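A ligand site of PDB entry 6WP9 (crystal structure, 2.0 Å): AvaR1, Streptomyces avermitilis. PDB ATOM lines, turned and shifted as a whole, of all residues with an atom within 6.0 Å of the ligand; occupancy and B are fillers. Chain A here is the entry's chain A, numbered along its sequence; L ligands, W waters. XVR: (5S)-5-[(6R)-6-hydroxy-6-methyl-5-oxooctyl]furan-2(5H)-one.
OG1 of Thr 142 lies within hydrogen-bond range of O16 of the ligand (2.7 Å).
The side-chain amide oxygen of Gln 176 sits close to an oxygen (O6) of the ligand (2.9 Å).
OG1 of Thr 142 is in hydrogen-bond range of O of Trp 138 (2.9 Å).
The indole nitrogen (NE1) of Trp 138 lies within hydrogen-bond range of the side-chain amide oxygen (OE1) of Gln 75, at 2.7 Å.
O of Val 169 sits at hydrogen-bond distance from OG1 of Thr 173, at 2.8 Å.
The side-chain hydroxyl (OG) of Ser 92 lies within hydrogen-bond range of the side-chain hydroxyl (OH) of Tyr 196 (2.8 Å).
NE2 of Gln 75 lies within hydrogen-bond range of OG1 of Thr 119 (2.9 Å).
O of Met 135 is in hydrogen-bond range of OG1 of Thr 139 (2.7 Å).
Gln 75 touches the ligand.
CD2 of Leu 99 touches C10 of the ligand (3.6 Å).
Val 116 touches the ligand (CG1 to O6, 3.6 Å).
CG2 of Val 120 touches C2 of the ligand, at 3.7 Å.
Met 135 touches the ligand (CE to C3, 3.8 Å).
CE3 of Trp 138 touches O15 of the ligand (3.3 Å).
O of Phe 168 touches C14 of the ligand, at 3.4 Å.
Val 169 touches the ligand.
Phe 172 touches the ligand (CD1 to O5, 3.96 Å).
Thr 173 touches the ligand.
OH of Tyr 196 touches C13 of the ligand, at 3.5 Å.
13 residues have an atom within 4 Å of the ligand: Gln 75, Leu 99, Val 116, Val 120, Met 135, Trp 138, Thr 142, Phe 168, Val 169, Phe 172, Thr 173, Gln 176 and Tyr 196.
The nearest printed residue that does not touch the ligand is His 141 (4.1 Å).
Water W1 lies within hydrogen-bond range of the side-chain hydroxyl (OG) of Ser 92, an oxygen (O16) of the ligand and the side-chain carboxylate (OE1) of Glu 95.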
ATOM      1  N   GLN A  75     -23.967  35.837  27.868  1.00  0.00           N
ATOM      2  CA  GLN A  75     -23.460  34.858  26.897  1.00  0.00           C
ATOM      3  C   GLN A  75     -22.966  35.423  25.558  1.00  0.00           C
ATOM      4  O   GLN A  75     -21.826  35.178  25.162  1.00  0.00           O
ATOM      5  CB  GLN A  75     -24.479  33.750  26.662  1.00  0.00           C
ATOM      6  CG  GLN A  75     -23.844  32.518  26.034  1.00  0.00           C
ATOM      7  CD  GLN A  75     -24.812  31.382  25.794  1.00  0.00           C
ATOM      8  OE1 GLN A  75     -25.024  30.982  24.647  1.00  0.00           O
ATOM      9  NE2 GLN A  75     -25.398  30.859  26.868  1.00  0.00           N
ATOM     10  N   LEU A  79     -18.676  36.891  23.916  1.00  0.00           N
ATOM     11  CA  LEU A  79     -18.009  36.468  22.693  1.00  0.00           C
ATOM     12  C   LEU A  79     -17.192  37.633  22.129  1.00  0.00           C
ATOM     13  O   LEU A  79     -17.763  38.664  21.793  1.00  0.00           O
ATOM     14  CB  LEU A  79     -19.048  35.968  21.677  1.00  0.00           C
ATOM     15  CG  LEU A  79     -18.747  35.202  20.380  1.00  0.00           C
ATOM     16  CD1 LEU A  79     -18.719  36.122  19.165  1.00  0.00           C
ATOM     17  CD2 LEU A  79     -17.534  34.279  20.428  1.00  0.00           C
ATOM     18  N   SER A  92     -19.545  35.457   9.866  1.00  0.00           N
ATOM     19  CA  SER A  92     -20.321  34.462  10.600  1.00  0.00           C
ATOM     20  C   SER A  92     -19.503  33.191  10.853  1.00  0.00           C
ATOM     21  O   SER A  92     -19.432  32.700  11.989  1.00  0.00           O
ATOM     22  CB  SER A  92     -21.617  34.148   9.857  1.00  0.00           C
ATOM     23  OG  SER A  92     -22.398  33.191  10.567  1.00  0.00           O
ATOM     24  N   GLU A  95     -16.944  33.814  13.461  1.00  0.00           N
ATOM     25  CA  GLU A  95     -17.595  33.785  14.789  1.00  0.00           C
ATOM     26  C   GLU A  95     -17.891  32.373  15.281  1.00  0.00           C
ATOM     27  O   GLU A  95     -17.657  32.063  16.456  1.00  0.00           O
ATOM     28  CB  GLU A  95     -18.892  34.566  14.768  1.00  0.00           C
ATOM     29  CG  GLU A  95     -18.710  36.063  14.680  1.00  0.00           C
ATOM     30  CD  GLU A  95     -20.033  36.795  14.678  1.00  0.00           C
ATOM     31  OE1 GLU A  95     -21.014  36.260  14.114  1.00  0.00           O
ATOM     32  OE2 GLU A  95     -20.088  37.913  15.242  1.00  0.00           O
ATOM     33  N   ALA A  96     -18.422  31.550  14.366  1.00  0.00           N
ATOM     34  CA  ALA A  96     -18.753  30.144  14.619  1.00  0.00           C
ATOM     35  C   ALA A  96     -17.536  29.338  15.050  1.00  0.00           C
ATOM     36  O   ALA A  96     -17.603  28.596  16.040  1.00  0.00           O
ATOM     37  CB  ALA A  96     -19.340  29.528  13.365  1.00  0.00           C
ATOM     38  N   LEU A  99     -16.165  30.709  18.498  1.00  0.00           N
ATOM     39  CA  LEU A  99     -16.983  30.125  19.562  1.00  0.00           C
ATOM     40  C   LEU A  99     -16.718  28.641  19.806  1.00  0.00           C
ATOM     41  O   LEU A  99     -16.687  28.210  20.953  1.00  0.00           O
ATOM     42  CB  LEU A  99     -18.490  30.366  19.332  1.00  0.00           C
ATOM     43  CG  LEU A  99     -19.514  29.925  20.390  1.00  0.00           C
ATOM     44  CD1 LEU A  99     -19.252  30.530  21.773  1.00  0.00           C
ATOM     45  CD2 LEU A  99     -20.925  30.268  19.943  1.00  0.00           C
ATOM     46  N   LEU A 103     -15.327  27.266  23.338  1.00  0.00           N
ATOM     47  CA  LEU A 103     -16.082  26.251  24.070  1.00  0.00           C
ATOM     48  C   LEU A 103     -15.214  25.040  24.401  1.00  0.00           C
ATOM     49  O   LEU A 103     -15.361  24.444  25.479  1.00  0.00           O
ATOM     50  CB  LEU A 103     -17.340  25.856  23.299  1.00  0.00           C
ATOM     51  CG  LEU A 103     -18.537  26.817  23.438  1.00  0.00           C
ATOM     52  CD1 LEU A 103     -19.585  26.474  22.388  1.00  0.00           C
ATOM     53  CD2 LEU A 103     -19.146  26.757  24.834  1.00  0.00           C
ATOM     54  N   VAL A 116     -23.365  28.167  28.581  1.00  0.00           N
ATOM     55  CA  VAL A 116     -23.943  27.161  27.661  1.00  0.00           C
ATOM     56  C   VAL A 116     -24.600  25.992  28.415  1.00  0.00           C
ATOM     57  O   VAL A 116     -25.732  25.584  28.084  1.00  0.00           O
ATOM     58  CB  VAL A 116     -22.907  26.718  26.599  1.00  0.00           C
ATOM     59  CG1 VAL A 116     -23.309  25.411  25.927  1.00  0.00           C
ATOM     60  CG2 VAL A 116     -22.735  27.822  25.567  1.00  0.00           C
ATOM     61  N   THR A 119     -27.896  27.081  29.691  1.00  0.00           N
ATOM     62  CA  THR A 119     -28.833  27.178  28.580  1.00  0.00           C
ATOM     63  C   THR A 119     -29.350  25.798  28.136  1.00  0.00           C
ATOM     64  O   THR A 119     -30.543  25.642  27.839  1.00  0.00           O
ATOM     65  CB  THR A 119     -28.194  27.859  27.350  1.00  0.00           C
ATOM     66  OG1 THR A 119     -27.475  29.032  27.755  1.00  0.00           O
ATOM     67  CG2 THR A 119     -29.250  28.220  26.300  1.00  0.00           C
ATOM     68  N   VAL A 120     -28.442  24.814  28.093  1.00  0.00           N
ATOM     69  CA  VAL A 120     -28.732  23.519  27.495  1.00  0.00           C
ATOM     70  C   VAL A 120     -29.380  22.532  28.473  1.00  0.00           C
ATOM     71  O   VAL A 120     -30.359  21.875  28.104  1.00  0.00           O
ATOM     72  CB  VAL A 120     -27.492  22.954  26.761  1.00  0.00           C
ATOM     73  CG1 VAL A 120     -27.765  21.572  26.190  1.00  0.00           C
ATOM     74  CG2 VAL A 120     -27.109  23.875  25.616  1.00  0.00           C
ATOM     75  N   MET A 135     -30.589  32.461  23.799  1.00  0.00           N
ATOM     76  CA  MET A 135     -31.016  31.870  22.531  1.00  0.00           C
ATOM     77  C   MET A 135     -31.646  32.922  21.602  1.00  0.00           C
ATOM     78  O   MET A 135     -31.433  32.894  20.385  1.00  0.00           O
ATOM     79  CB  MET A 135     -31.964  30.689  22.759  1.00  0.00           C
ATOM     80  CG  MET A 135     -31.318  29.390  23.213  1.00  0.00           C
ATOM     81  SD  MET A 135     -29.785  28.977  22.370  1.00  0.00           S
ATOM     82  CE  MET A 135     -29.832  27.181  22.428  1.00  0.00           C
ATOM     83  N   TRP A 138     -28.700  35.229  20.447  1.00  0.00           N
ATOM     84  CA  TRP A 138     -27.961  34.609  19.335  1.00  0.00           C
ATOM     85  C   TRP A 138     -28.744  34.643  18.024  1.00  0.00           C
ATOM     86  O   TRP A 138     -28.148  34.847  16.971  1.00  0.00           O
ATOM     87  CB  TRP A 138     -27.566  33.165  19.637  1.00  0.00           C
ATOM     88  CG  TRP A 138     -26.403  32.998  20.560  1.00  0.00           C
ATOM     89  CD1 TRP A 138     -26.419  32.380  21.773  1.00  0.00           C
ATOM     90  CD2 TRP A 138     -25.058  33.434  20.359  1.00  0.00           C
ATOM     91  NE1 TRP A 138     -25.172  32.403  22.340  1.00  0.00           N
ATOM     92  CE2 TRP A 138     -24.313  33.039  21.489  1.00  0.00           C
ATOM     93  CE3 TRP A 138     -24.403  34.123  19.309  1.00  0.00           C
ATOM     94  CZ2 TRP A 138     -22.935  33.317  21.624  1.00  0.00           C
ATOM     95  CZ3 TRP A 138     -23.035  34.390  19.437  1.00  0.00           C
ATOM     96  CH2 TRP A 138     -22.315  33.987  20.601  1.00  0.00           C
ATOM     97  N   THR A 139     -30.052  34.429  18.106  1.00  0.00           N
ATOM     98  CA  THR A 139     -30.907  34.462  16.918  1.00  0.00           C
ATOM     99  C   THR A 139     -30.936  35.857  16.282  1.00  0.00           C
ATOM    100  O   THR A 139     -30.839  35.985  15.056  1.00  0.00           O
ATOM    101  CB  THR A 139     -32.334  33.923  17.233  1.00  0.00           C
ATOM    102  OG1 THR A 139     -32.224  32.616  17.817  1.00  0.00           O
ATOM    103  CG2 THR A 139     -33.171  33.827  15.943  1.00  0.00           C
ATOM    104  N   HIS A 141     -28.674  38.271  16.730  1.00  0.00           N
ATOM    105  CA  HIS A 141     -27.304  38.481  16.254  1.00  0.00           C
ATOM    106  C   HIS A 141     -27.072  37.863  14.860  1.00  0.00           C
ATOM    107  O   HIS A 141     -26.586  38.530  13.959  1.00  0.00           O
ATOM    108  CB  HIS A 141     -26.282  37.953  17.254  1.00  0.00           C
ATOM    109  CG  HIS A 141     -24.895  37.905  16.710  1.00  0.00           C
ATOM    110  ND1 HIS A 141     -24.033  38.970  16.770  1.00  0.00           N
ATOM    111  CD2 HIS A 141     -24.214  36.898  16.093  1.00  0.00           C
ATOM    112  CE1 HIS A 141     -22.883  38.641  16.218  1.00  0.00           C
ATOM    113  NE2 HIS A 141     -22.965  37.391  15.799  1.00  0.00           N
ATOM    114  N   THR A 142     -27.425  36.579  14.718  1.00  0.00           N
ATOM    115  CA  THR A 142     -27.228  35.834  13.475  1.00  0.00           C
ATOM    116  C   THR A 142     -28.138  36.353  12.347  1.00  0.00           C
ATOM    117  O   THR A 142     -27.705  36.461  11.195  1.00  0.00           O
ATOM    118  CB  THR A 142     -27.397  34.322  13.714  1.00  0.00           C
ATOM    119  OG1 THR A 142     -26.502  33.915  14.762  1.00  0.00           O
ATOM    120  CG2 THR A 142     -27.080  33.499  12.451  1.00  0.00           C
ATOM    121  N   ALA A 165     -31.407  32.076  10.600  1.00  0.00           N
ATOM    122  CA  ALA A 165     -30.825  32.375  11.907  1.00  0.00           C
ATOM    123  C   ALA A 165     -31.183  31.281  12.914  1.00  0.00           C
ATOM    124  O   ALA A 165     -30.295  30.704  13.553  1.00  0.00           O
ATOM    125  CB  ALA A 165     -31.272  33.751  12.391  1.00  0.00           C
ATOM    126  N   PHE A 168     -29.339  28.095  12.064  1.00  0.00           N
ATOM    127  CA  PHE A 168     -27.921  28.125  12.421  1.00  0.00           C
ATOM    128  C   PHE A 168     -27.674  28.069  13.935  1.00  0.00           C
ATOM    129  O   PHE A 168     -26.754  27.372  14.358  1.00  0.00           O
ATOM    130  CB  PHE A 168     -27.218  29.337  11.778  1.00  0.00           C
ATOM    131  CG  PHE A 168     -26.679  29.055  10.397  1.00  0.00           C
ATOM    132  CD1 PHE A 168     -27.539  28.986   9.301  1.00  0.00           C
ATOM    133  CD2 PHE A 168     -25.316  28.829  10.210  1.00  0.00           C
ATOM    134  CE1 PHE A 168     -27.045  28.722   8.026  1.00  0.00           C
ATOM    135  CE2 PHE A 168     -24.822  28.555   8.936  1.00  0.00           C
ATOM    136  CZ  PHE A 168     -25.681  28.508   7.848  1.00  0.00           C
ATOM    137  N   VAL A 169     -28.477  28.806  14.709  1.00  0.00           N
ATOM    138  CA  VAL A 169     -28.349  28.810  16.173  1.00  0.00           C
ATOM    139  C   VAL A 169     -28.666  27.414  16.727  1.00  0.00           C
ATOM    140  O   VAL A 169     -27.913  26.889  17.554  1.00  0.00           O
ATOM    141  CB  VAL A 169     -29.228  29.916  16.839  1.00  0.00           C
ATOM    142  CG1 VAL A 169     -29.132  29.833  18.347  1.00  0.00           C
ATOM    143  CG2 VAL A 169     -28.802  31.298  16.402  1.00  0.00           C
ATOM    144  N   PHE A 172     -25.945  24.719  15.404  1.00  0.00           N
ATOM    145  CA  PHE A 172     -24.678  24.950  16.139  1.00  0.00           C
ATOM    146  C   PHE A 172     -24.707  24.339  17.536  1.00  0.00           C
ATOM    147  O   PHE A 172     -23.747  23.643  17.954  1.00  0.00           O
ATOM    148  CB  PHE A 172     -24.297  26.462  16.234  1.00  0.00           C
ATOM    149  CG  PHE A 172     -22.950  26.699  16.896  1.00  0.00           C
ATOM    150  CD1 PHE A 172     -22.813  26.697  18.288  1.00  0.00           C
ATOM    151  CD2 PHE A 172     -21.816  26.880  16.122  1.00  0.00           C
ATOM    152  CE1 PHE A 172     -21.575  26.873  18.881  1.00  0.00           C
ATOM    153  CE2 PHE A 172     -20.569  27.077  16.711  1.00  0.00           C
ATOM    154  CZ  PHE A 172     -20.453  27.073  18.096  1.00  0.00           C
ATOM    155  N   THR A 173     -25.801  24.616  18.247  1.00  0.00           N
ATOM    156  CA  THR A 173     -26.041  24.113  19.604  1.00  0.00           C
ATOM    157  C   THR A 173     -25.945  22.594  19.653  1.00  0.00           C
ATOM    158  O   THR A 173     -25.312  22.041  20.551  1.00  0.00           O
ATOM    159  CB  THR A 173     -27.422  24.602  20.122  1.00  0.00           C
ATOM    160  OG1 THR A 173     -27.405  26.038  20.207  1.00  0.00           O
ATOM    161  CG2 THR A 173     -27.766  24.008  21.513  1.00  0.00           C
ATOM    162  N   GLY A 174     -26.550  21.933  18.671  1.00  0.00           N
ATOM    163  CA  GLY A 174     -26.543  20.470  18.616  1.00  0.00           C
ATOM    164  C   GLY A 174     -25.204  19.866  18.268  1.00  0.00           C
ATOM    165  O   GLY A 174     -24.817  18.852  18.863  1.00  0.00           O
ATOM    166  N   GLN A 176     -22.392  21.329  18.854  1.00  0.00           N
ATOM    167  CA  GLN A 176     -21.739  21.519  20.141  1.00  0.00           C
ATOM    168  C   GLN A 176     -22.029  20.365  21.123  1.00  0.00           C
ATOM    169  O   GLN A 176     -21.093  19.791  21.674  1.00  0.00           O
ATOM    170  CB  GLN A 176     -22.148  22.878  20.743  1.00  0.00           C
ATOM    171  CG  GLN A 176     -21.422  23.270  22.018  1.00  0.00           C
ATOM    172  CD  GLN A 176     -21.970  22.551  23.239  1.00  0.00           C
ATOM    173  OE1 GLN A 176     -23.160  22.614  23.539  1.00  0.00           O
ATOM    174  NE2 GLN A 176     -21.111  21.837  23.927  1.00  0.00           N
ATOM    175  N   VAL A 177     -23.315  20.063  21.333  1.00  0.00           N
ATOM    176  CA  VAL A 177     -23.756  19.010  22.267  1.00  0.00           C
ATOM    177  C   VAL A 177     -23.215  17.636  21.870  1.00  0.00           C
ATOM    178  O   VAL A 177     -22.716  16.902  22.715  1.00  0.00           O
ATOM    179  CB  VAL A 177     -25.298  18.955  22.428  1.00  0.00           C
ATOM    180  CG1 VAL A 177     -25.738  17.678  23.130  1.00  0.00           C
ATOM    181  CG2 VAL A 177     -25.800  20.175  23.200  1.00  0.00           C
ATOM    182  N   TYR A 196     -21.337  24.495   8.361  1.00  0.00           N
ATOM    183  CA  TYR A 196     -21.388  25.644   7.469  1.00  0.00           C
ATOM    184  C   TYR A 196     -21.230  25.219   6.016  1.00  0.00           C
ATOM    185  O   TYR A 196     -21.966  25.722   5.169  1.00  0.00           O
ATOM    186  CB  TYR A 196     -20.346  26.696   7.849  1.00  0.00           C
ATOM    187  CG  TYR A 196     -20.855  27.734   8.813  1.00  0.00           C
ATOM    188  CD1 TYR A 196     -21.196  27.395  10.127  1.00  0.00           C
ATOM    189  CD2 TYR A 196     -20.977  29.079   8.420  1.00  0.00           C
ATOM    190  CE1 TYR A 196     -21.663  28.347  11.023  1.00  0.00           C
ATOM    191  CE2 TYR A 196     -21.444  30.041   9.315  1.00  0.00           C
ATOM    192  CZ  TYR A 196     -21.778  29.670  10.610  1.00  0.00           C
ATOM    193  OH  TYR A 196     -22.233  30.603  11.507  1.00  0.00           O
HETATM  194  O15 XVR L   1     -25.503  32.138  16.889  1.00  0.00           O
HETATM  195  C11 XVR L   1     -24.391  31.596  16.863  1.00  0.00           C
HETATM  196  C12 XVR L   1     -23.461  31.872  15.692  1.00  0.00           C
HETATM  197  O16 XVR L   1     -24.020  32.940  14.904  1.00  0.00           O
HETATM  198  C13 XVR L   1     -23.259  30.638  14.803  1.00  0.00           C
HETATM  199  C14 XVR L   1     -24.525  29.951  14.337  1.00  0.00           C
HETATM  200  C10 XVR L   1     -23.960  30.654  17.972  1.00  0.00           C
HETATM  201  C9  XVR L   1     -25.141  30.101  18.770  1.00  0.00           C
HETATM  202  C8  XVR L   1     -24.632  29.721  20.157  1.00  0.00           C
HETATM  203  C7  XVR L   1     -25.659  28.910  20.928  1.00  0.00           C
HETATM  204  C4  XVR L   1     -25.055  28.428  22.250  1.00  0.00           C
HETATM  205  C3  XVR L   1     -26.132  27.868  23.146  1.00  0.00           C
HETATM  206  C2  XVR L   1     -25.967  26.568  23.355  1.00  0.00           C
HETATM  207  O5  XVR L   1     -24.172  27.338  21.957  1.00  0.00           O
HETATM  208  C1  XVR L   1     -24.765  26.201  22.607  1.00  0.00           C
HETATM  209  O6  XVR L   1     -24.287  25.095  22.507  1.00  0.00           O
HETATM  210  C5  XVR L   1     -22.082  32.336  16.194  1.00  0.00           C
HETATM  211  O   HOH W   1     -22.919  34.492  12.918  1.00  0.00           O
